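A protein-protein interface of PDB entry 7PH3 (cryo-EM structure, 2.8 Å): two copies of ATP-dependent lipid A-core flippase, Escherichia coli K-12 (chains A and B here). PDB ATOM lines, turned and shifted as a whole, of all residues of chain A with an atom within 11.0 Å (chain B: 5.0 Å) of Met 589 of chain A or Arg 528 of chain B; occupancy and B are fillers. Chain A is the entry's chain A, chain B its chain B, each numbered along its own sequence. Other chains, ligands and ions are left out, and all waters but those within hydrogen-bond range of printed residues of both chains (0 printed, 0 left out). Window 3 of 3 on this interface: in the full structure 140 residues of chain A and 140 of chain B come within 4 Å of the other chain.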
ATOM      1  N   GLY A 387       7.989  24.843  24.544  1.00  0.00           N
ATOM      2  CA  GLY A 387       7.190  25.750  25.341  1.00  0.00           C
ATOM      3  C   GLY A 387       7.047  27.079  24.639  1.00  0.00           C
ATOM      4  O   GLY A 387       7.771  27.405  23.708  1.00  0.00           O
ATOM      5  N   ARG A 388       6.085  27.859  25.108  1.00  0.00           N
ATOM      6  CA  ARG A 388       5.811  29.152  24.512  1.00  0.00           C
ATOM      7  C   ARG A 388       6.968  30.121  24.728  1.00  0.00           C
ATOM      8  O   ARG A 388       7.895  29.877  25.499  1.00  0.00           O
ATOM      9  CB  ARG A 388       4.527  29.742  25.080  1.00  0.00           C
ATOM     10  CG  ARG A 388       3.416  28.754  25.229  1.00  0.00           C
ATOM     11  CD  ARG A 388       2.139  29.490  25.488  1.00  0.00           C
ATOM     12  NE  ARG A 388       1.679  30.154  24.278  1.00  0.00           N
ATOM     13  CZ  ARG A 388       0.729  31.077  24.255  1.00  0.00           C
ATOM     14  NH1 ARG A 388       0.382  31.640  23.110  1.00  0.00           N
ATOM     15  NH2 ARG A 388       0.131  31.436  25.381  1.00  0.00           N
ATOM     16  N   SER A 389       6.898  31.238  24.020  1.00  0.00           N
ATOM     17  CA  SER A 389       7.913  32.266  24.144  1.00  0.00           C
ATOM     18  C   SER A 389       7.901  32.866  25.541  1.00  0.00           C
ATOM     19  O   SER A 389       6.841  33.115  26.118  1.00  0.00           O
ATOM     20  CB  SER A 389       7.687  33.350  23.097  1.00  0.00           C
ATOM     21  OG  SER A 389       7.864  32.835  21.800  1.00  0.00           O
ATOM     22  N   HIS A 548      10.758  25.537  18.628  1.00  0.00           N
ATOM     23  CA  HIS A 548       9.364  26.049  18.673  1.00  0.00           C
ATOM     24  C   HIS A 548       8.608  25.239  17.616  1.00  0.00           C
ATOM     25  O   HIS A 548       7.370  25.368  17.541  1.00  0.00           O
ATOM     26  CB  HIS A 548       9.326  27.555  18.384  1.00  0.00           C
ATOM     27  CG  HIS A 548       9.174  28.394  19.607  1.00  0.00           C
ATOM     28  ND1 HIS A 548       8.178  28.176  20.536  1.00  0.00           N
ATOM     29  CD2 HIS A 548       9.885  29.450  20.055  1.00  0.00           C
ATOM     30  CE1 HIS A 548       8.283  29.062  21.505  1.00  0.00           C
ATOM     31  NE2 HIS A 548       9.322  29.853  21.235  1.00  0.00           N
ATOM     32  N   ARG A 549       9.343  24.432  16.838  1.00  0.00           N
ATOM     33  CA  ARG A 549       8.731  23.568  15.791  1.00  0.00           C
ATOM     34  C   ARG A 549       8.872  22.114  16.250  1.00  0.00           C
ATOM     35  O   ARG A 549       9.986  21.740  16.662  1.00  0.00           O
ATOM     36  CB  ARG A 549       9.461  23.750  14.456  1.00  0.00           C
ATOM     37  CG  ARG A 549       9.573  25.193  13.987  1.00  0.00           C
ATOM     38  CD  ARG A 549      10.405  25.289  12.722  1.00  0.00           C
ATOM     39  NE  ARG A 549      10.529  26.650  12.220  1.00  0.00           N
ATOM     40  CZ  ARG A 549      11.189  26.986  11.117  1.00  0.00           C
ATOM     41  NH1 ARG A 549      11.245  28.251  10.739  1.00  0.00           N
ATOM     42  NH2 ARG A 549      11.789  26.055  10.396  1.00  0.00           N
ATOM     43  N   LEU A 550       7.798  21.324  16.176  1.00  0.00           N
ATOM     44  CA  LEU A 550       7.852  19.942  16.728  1.00  0.00           C
ATOM     45  C   LEU A 550       8.391  18.934  15.702  1.00  0.00           C
ATOM     46  O   LEU A 550       8.786  17.831  16.134  1.00  0.00           O
ATOM     47  CB  LEU A 550       6.460  19.555  17.239  1.00  0.00           C
ATOM     48  CG  LEU A 550       5.869  20.514  18.271  1.00  0.00           C
ATOM     49  CD1 LEU A 550       4.568  19.969  18.830  1.00  0.00           C
ATOM     50  CD2 LEU A 550       6.854  20.780  19.399  1.00  0.00           C
ATOM     51  N   SER A 551       8.419  19.282  14.411  1.00  0.00           N
ATOM     52  CA  SER A 551       8.995  18.372  13.435  1.00  0.00           C
ATOM     53  C   SER A 551      10.491  18.213  13.631  1.00  0.00           C
ATOM     54  O   SER A 551      11.057  17.197  13.216  1.00  0.00           O
ATOM     55  CB  SER A 551       8.703  18.862  12.019  1.00  0.00           C
ATOM     56  OG  SER A 551       7.314  18.830  11.753  1.00  0.00           O
ATOM     57  N   LEU A 577       1.954  12.159  23.018  1.00  0.00           N
ATOM     58  CA  LEU A 577       0.790  12.263  22.147  1.00  0.00           C
ATOM     59  C   LEU A 577      -0.379  11.477  22.703  1.00  0.00           C
ATOM     60  O   LEU A 577      -1.536  11.833  22.459  1.00  0.00           O
ATOM     61  CB  LEU A 577       1.125  11.783  20.738  1.00  0.00           C
ATOM     62  CG  LEU A 577       1.716  12.845  19.823  1.00  0.00           C
ATOM     63  CD1 LEU A 577       1.834  12.302  18.420  1.00  0.00           C
ATOM     64  CD2 LEU A 577       0.874  14.103  19.849  1.00  0.00           C
ATOM     65  N   GLY A 581      -2.045  15.912  26.940  1.00  0.00           N
ATOM     66  CA  GLY A 581      -1.744  17.111  27.698  1.00  0.00           C
ATOM     67  C   GLY A 581      -1.285  18.276  26.846  1.00  0.00           C
ATOM     68  O   GLY A 581      -1.733  18.433  25.710  1.00  0.00           O
ATOM     69  N   VAL A 582      -0.378  19.090  27.386  1.00  0.00           N
ATOM     70  CA  VAL A 582       0.042  20.319  26.713  1.00  0.00           C
ATOM     71  C   VAL A 582       0.711  20.005  25.383  1.00  0.00           C
ATOM     72  O   VAL A 582       0.450  20.656  24.363  1.00  0.00           O
ATOM     73  CB  VAL A 582       0.969  21.134  27.632  1.00  0.00           C
ATOM     74  CG1 VAL A 582       1.382  22.422  26.966  1.00  0.00           C
ATOM     75  CG2 VAL A 582       0.281  21.418  28.944  1.00  0.00           C
ATOM     76  N   TYR A 583       1.589  19.005  25.370  1.00  0.00           N
ATOM     77  CA  TYR A 583       2.270  18.663  24.132  1.00  0.00           C
ATOM     78  C   TYR A 583       1.289  18.177  23.076  1.00  0.00           C
ATOM     79  O   TYR A 583       1.476  18.449  21.887  1.00  0.00           O
ATOM     80  CB  TYR A 583       3.357  17.622  24.391  1.00  0.00           C
ATOM     81  CG  TYR A 583       4.095  17.238  23.142  1.00  0.00           C
ATOM     82  CD1 TYR A 583       5.129  18.019  22.662  1.00  0.00           C
ATOM     83  CD2 TYR A 583       3.751  16.100  22.431  1.00  0.00           C
ATOM     84  CE1 TYR A 583       5.795  17.683  21.514  1.00  0.00           C
ATOM     85  CE2 TYR A 583       4.416  15.754  21.283  1.00  0.00           C
ATOM     86  CZ  TYR A 583       5.435  16.550  20.831  1.00  0.00           C
ATOM     87  OH  TYR A 583       6.103  16.206  19.684  1.00  0.00           O
ATOM     88  N   ALA A 584       0.234  17.472  23.486  1.00  0.00           N
ATOM     89  CA  ALA A 584      -0.785  17.053  22.532  1.00  0.00           C
ATOM     90  C   ALA A 584      -1.455  18.252  21.877  1.00  0.00           C
ATOM     91  O   ALA A 584      -1.672  18.258  20.661  1.00  0.00           O
ATOM     92  CB  ALA A 584      -1.822  16.170  23.221  1.00  0.00           C
ATOM     93  N   GLN A 585      -1.790  19.277  22.661  1.00  0.00           N
ATOM     94  CA  GLN A 585      -2.348  20.496  22.097  1.00  0.00           C
ATOM     95  C   GLN A 585      -1.385  21.214  21.167  1.00  0.00           C
ATOM     96  O   GLN A 585      -1.811  21.678  20.106  1.00  0.00           O
ATOM     97  CB  GLN A 585      -2.777  21.456  23.203  1.00  0.00           C
ATOM     98  CG  GLN A 585      -4.209  21.284  23.653  1.00  0.00           C
ATOM     99  CD  GLN A 585      -4.331  20.449  24.905  1.00  0.00           C
ATOM    100  OE1 GLN A 585      -3.782  20.798  25.951  1.00  0.00           O
ATOM    101  NE2 GLN A 585      -5.048  19.337  24.807  1.00  0.00           N
ATOM    102  N   LEU A 586      -0.109  21.326  21.533  1.00  0.00           N
ATOM    103  CA  LEU A 586       0.845  21.963  20.631  1.00  0.00           C
ATOM    104  C   LEU A 586       0.958  21.198  19.323  1.00  0.00           C
ATOM    105  O   LEU A 586       0.989  21.797  18.244  1.00  0.00           O
ATOM    106  CB  LEU A 586       2.216  22.063  21.287  1.00  0.00           C
ATOM    107  CG  LEU A 586       2.280  22.697  22.663  1.00  0.00           C
ATOM    108  CD1 LEU A 586       3.566  22.272  23.339  1.00  0.00           C
ATOM    109  CD2 LEU A 586       2.202  24.195  22.529  1.00  0.00           C
ATOM    110  N   HIS A 587       1.035  19.874  19.401  1.00  0.00           N
ATOM    111  CA  HIS A 587       1.175  19.069  18.197  1.00  0.00           C
ATOM    112  C   HIS A 587      -0.073  19.156  17.330  1.00  0.00           C
ATOM    113  O   HIS A 587       0.022  19.217  16.101  1.00  0.00           O
ATOM    114  CB  HIS A 587       1.478  17.624  18.584  1.00  0.00           C
ATOM    115  CG  HIS A 587       1.873  16.759  17.433  1.00  0.00           C
ATOM    116  ND1 HIS A 587       3.185  16.552  17.077  1.00  0.00           N
ATOM    117  CD2 HIS A 587       1.127  16.046  16.558  1.00  0.00           C
ATOM    118  CE1 HIS A 587       3.232  15.748  16.032  1.00  0.00           C
ATOM    119  NE2 HIS A 587       1.997  15.427  15.696  1.00  0.00           N
ATOM    120  N   LYS A 588      -1.250  19.165  17.953  1.00  0.00           N
ATOM    121  CA  LYS A 588      -2.488  19.238  17.190  1.00  0.00           C
ATOM    122  C   LYS A 588      -2.605  20.564  16.454  1.00  0.00           C
ATOM    123  O   LYS A 588      -3.036  20.603  15.297  1.00  0.00           O
ATOM    124  CB  LYS A 588      -3.686  19.031  18.113  1.00  0.00           C
ATOM    125  CG  LYS A 588      -5.011  18.947  17.380  1.00  0.00           C
ATOM    126  CD  LYS A 588      -6.182  19.089  18.331  1.00  0.00           C
ATOM    127  CE  LYS A 588      -7.500  18.961  17.594  1.00  0.00           C
ATOM    128  NZ  LYS A 588      -7.705  17.577  17.087  1.00  0.00           N
ATOM    129  N   MET A 589      -2.230  21.660  17.103  1.00  0.00           N
ATOM    130  CA  MET A 589      -2.372  22.974  16.494  1.00  0.00           C
ATOM    131  C   MET A 589      -1.197  23.341  15.605  1.00  0.00           C
ATOM    132  O   MET A 589      -1.210  24.417  15.005  1.00  0.00           O
ATOM    133  CB  MET A 589      -2.575  24.039  17.574  1.00  0.00           C
ATOM    134  CG  MET A 589      -1.353  24.340  18.403  1.00  0.00           C
ATOM    135  SD  MET A 589      -1.457  25.940  19.212  1.00  0.00           S
ATOM    136  CE  MET A 589      -1.918  26.982  17.838  1.00  0.00           C
ATOM    137  N   GLN A 590      -0.199  22.478  15.494  1.00  0.00           N
ATOM    138  CA  GLN A 590       0.883  22.668  14.537  1.00  0.00           C
ATOM    139  C   GLN A 590       0.751  21.672  13.394  1.00  0.00           C
ATOM    140  O   GLN A 590      -0.202  20.900  13.331  1.00  0.00           O
ATOM    141  CB  GLN A 590       2.241  22.510  15.215  1.00  0.00           C
ATOM    142  CG  GLN A 590       3.247  23.559  14.826  1.00  0.00           C
ATOM    143  CD  GLN A 590       4.586  23.351  15.490  1.00  0.00           C
ATOM    144  OE1 GLN A 590       5.472  22.709  14.934  1.00  0.00           O
ATOM    145  NE2 GLN A 590       4.743  23.895  16.688  1.00  0.00           N
ATOM    146  N   THR B 524       3.397  28.526  18.029  1.00  0.00           N
ATOM    147  CA  THR B 524       2.267  28.474  17.102  1.00  0.00           C
ATOM    148  C   THR B 524       1.078  29.301  17.582  1.00  0.00           C
ATOM    149  O   THR B 524       0.456  30.019  16.793  1.00  0.00           O
ATOM    150  CB  THR B 524       1.852  27.018  16.880  1.00  0.00           C
ATOM    151  OG1 THR B 524       3.022  26.217  16.703  1.00  0.00           O
ATOM    152  CG2 THR B 524       0.988  26.884  15.647  1.00  0.00           C
ATOM    153  N   GLU B 525       0.752  29.223  18.873  1.00  0.00           N
ATOM    154  CA  GLU B 525      -0.403  29.954  19.387  1.00  0.00           C
ATOM    155  C   GLU B 525      -0.173  31.460  19.346  1.00  0.00           C
ATOM    156  O   GLU B 525      -1.084  32.232  19.016  1.00  0.00           O
ATOM    157  CB  GLU B 525      -0.723  29.483  20.805  1.00  0.00           C
ATOM    158  CG  GLU B 525      -2.108  29.872  21.286  1.00  0.00           C
ATOM    159  CD  GLU B 525      -2.256  29.793  22.794  1.00  0.00           C
ATOM    160  OE1 GLU B 525      -2.696  30.790  23.400  1.00  0.00           O
ATOM    161  OE2 GLU B 525      -1.947  28.731  23.372  1.00  0.00           O
ATOM    162  N   SER B 526       1.048  31.893  19.656  1.00  0.00           N
ATOM    163  CA  SER B 526       1.390  33.307  19.571  1.00  0.00           C
ATOM    164  C   SER B 526       1.269  33.819  18.139  1.00  0.00           C
ATOM    165  O   SER B 526       0.744  34.914  17.900  1.00  0.00           O
ATOM    166  CB  SER B 526       2.803  33.509  20.112  1.00  0.00           C
ATOM    167  OG  SER B 526       3.004  34.823  20.582  1.00  0.00           O
ATOM    168  N   GLU B 527       1.736  33.034  17.169  1.00  0.00           N
ATOM    169  CA  GLU B 527       1.631  33.448  15.775  1.00  0.00           C
ATOM    170  C   GLU B 527       0.187  33.474  15.313  1.00  0.00           C
ATOM    171  O   GLU B 527      -0.184  34.318  14.498  1.00  0.00           O
ATOM    172  CB  GLU B 527       2.442  32.519  14.883  1.00  0.00           C
ATOM    173  CG  GLU B 527       2.428  32.938  13.461  1.00  0.00           C
ATOM    174  CD  GLU B 527       1.168  32.522  12.751  1.00  0.00           C
ATOM    175  OE1 GLU B 527       0.529  31.540  13.181  1.00  0.00           O
ATOM    176  OE2 GLU B 527       0.849  33.147  11.725  1.00  0.00           O
ATOM    177  N   ARG B 528      -0.639  32.544  15.796  1.00  0.00           N
ATOM    178  CA  ARG B 528      -2.052  32.577  15.441  1.00  0.00           C
ATOM    179  C   ARG B 528      -2.714  33.841  15.966  1.00  0.00           C
ATOM    180  O   ARG B 528      -3.502  34.479  15.260  1.00  0.00           O
ATOM    181  CB  ARG B 528      -2.768  31.337  15.974  1.00  0.00           C
ATOM    182  CG  ARG B 528      -2.342  30.037  15.318  1.00  0.00           C
ATOM    183  CD  ARG B 528      -3.421  29.462  14.430  1.00  0.00           C
ATOM    184  NE  ARG B 528      -4.252  28.490  15.134  1.00  0.00           N
ATOM    185  CZ  ARG B 528      -4.032  27.180  15.141  1.00  0.00           C
ATOM    186  NH1 ARG B 528      -4.842  26.374  15.807  1.00  0.00           N
ATOM    187  NH2 ARG B 528      -2.996  26.674  14.491  1.00  0.00           N
ATOM    188  N   ALA B 529      -2.398  34.225  17.204  1.00  0.00           N
ATOM    189  CA  ALA B 529      -2.945  35.466  17.743  1.00  0.00           C
ATOM    190  C   ALA B 529      -2.500  36.671  16.924  1.00  0.00           C
ATOM    191  O   ALA B 529      -3.317  37.540  16.574  1.00  0.00           O
ATOM    192  CB  ALA B 529      -2.523  35.627  19.197  1.00  0.00           C
ATOM    193  N   ILE B 530      -1.210  36.734  16.599  1.00  0.00           N
ATOM    194  CA  ILE B 530      -0.698  37.852  15.816  1.00  0.00           C
ATOM    195  C   ILE B 530      -1.344  37.879  14.439  1.00  0.00           C
ATOM    196  O   ILE B 530      -1.678  38.946  13.916  1.00  0.00           O
ATOM    197  CB  ILE B 530       0.836  37.775  15.738  1.00  0.00           C
ATOM    198  CG1 ILE B 530       1.430  37.986  17.132  1.00  0.00           C
ATOM    199  CG2 ILE B 530       1.373  38.773  14.744  1.00  0.00           C
ATOM    200  CD1 ILE B 530       2.891  37.681  17.245  1.00  0.00           C
ATOM    201  N   GLN B 531      -1.540  36.708  13.836  1.00  0.00           N
ATOM    202  CA  GLN B 531      -2.159  36.622  12.520  1.00  0.00           C
ATOM    203  C   GLN B 531      -3.608  37.075  12.560  1.00  0.00           C
ATOM    204  O   GLN B 531      -4.093  37.700  11.615  1.00  0.00           O
ATOM    205  CB  GLN B 531      -2.057  35.190  11.999  1.00  0.00           C
ATOM    206  CG  GLN B 531      -2.727  34.954  10.667  1.00  0.00           C
ATOM    207  CD  GLN B 531      -2.050  35.706   9.554  1.00  0.00           C
ATOM    208  OE1 GLN B 531      -0.850  35.569   9.336  1.00  0.00           O
ATOM    209  NE2 GLN B 531      -2.821  36.509   8.834  1.00  0.00           N
ATOM    210  N   ALA B 532      -4.323  36.750  13.635  1.00  0.00           N
ATOM    211  CA  ALA B 532      -5.692  37.235  13.780  1.00  0.00           C
ATOM    212  C   ALA B 532      -5.727  38.755  13.869  1.00  0.00           C
ATOM    213  O   ALA B 532      -6.568  39.406  13.238  1.00  0.00           O
ATOM    214  CB  ALA B 532      -6.338  36.608  15.012  1.00  0.00           C
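Among the printed residues, merely in contact across the chains: Met 589 of chain A with Thr 524 of chain B (3.4 Å), Arg 388 of chain A with Ser 526 of chain B (3.5 Å) and Met 589 of chain A with Glu 525 of chain B (3.6 Å).
Printed residues of chain B within 4 Å of Arg 388 of chain A: Glu 525 and Ser 526. Of the printed residues of chain B, Gln 590 of chain A touches Thr 524. Thr 524 of chain B touches just these residues of chain A: Met 589 and Gln 590. Of the printed residues of chain A, Ser 526 of chain B touches Arg 388 (3.5 Å). Glu 527 of chain B touches none of the printed residues of chain A. Arg 528 of chain B touches just one residue of chain A: Met 589. Ala 529 of chain B touches none of the printed residues of chain A. No residue of chain A comes within 4 Å of Ile 530 of chain B. No residue of chain A comes within 4 Å of Gln 531 of chain B. No residue of chain A comes within 4 Å of Ala 532 of chain B. The nearest printed residue of chain B that does not touch Arg 388 of chain A is Thr 524 of chain B (6.0 Å).
No position is printed for both chains. Of the 6 pairs that touch across the chains among the printed residues, none has its exchanged pair printed and touching as well.
O of His 548 of chain A lies within hydrogen-bond range of NE2 of Gln 590 of chain A (3.1 Å). OE1 of Gln 590 of chain A sits at hydrogen-bond distance from N of Leu 550 of chain A (3.0 Å).
The side-chain carboxylate (OE1) of Glu 525 of chain B lies within salt-bridge range of the guanidinium group (NH1) of Arg 388 of chain A, 3.2 Å away. NH2 of Arg 528 of chain B sits at hydrogen-bond distance from O of Met 589 of chain A (2.9 Å). NE2 of Gln 590 of chain A lies within hydrogen-bond range of OG1 of Thr 524 of chain B, 2.9 Å away.
Of the 9 printed residues of chain B, 4 touch a printed residue of chain A. Printed residues of chain B that touch a printed residue of chain A: Thr 524, Glu 525, Ser 526 and Arg 528. Of the 18 printed residues of chain A, 3 touch a printed residue of chain B. Hydrophobic or aromatic side chains of chain A within 4 Å of the printed part of chain B: Met 589. Among the printed residues, 6 pairs touch across the chains. Among the printed residues, Asp or Glu carboxylates within 4 Å of a Lys or Arg side-chain nitrogen of the other chain: Arg 388 of chain A with Glu 525 of chain B (3.2 Å).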
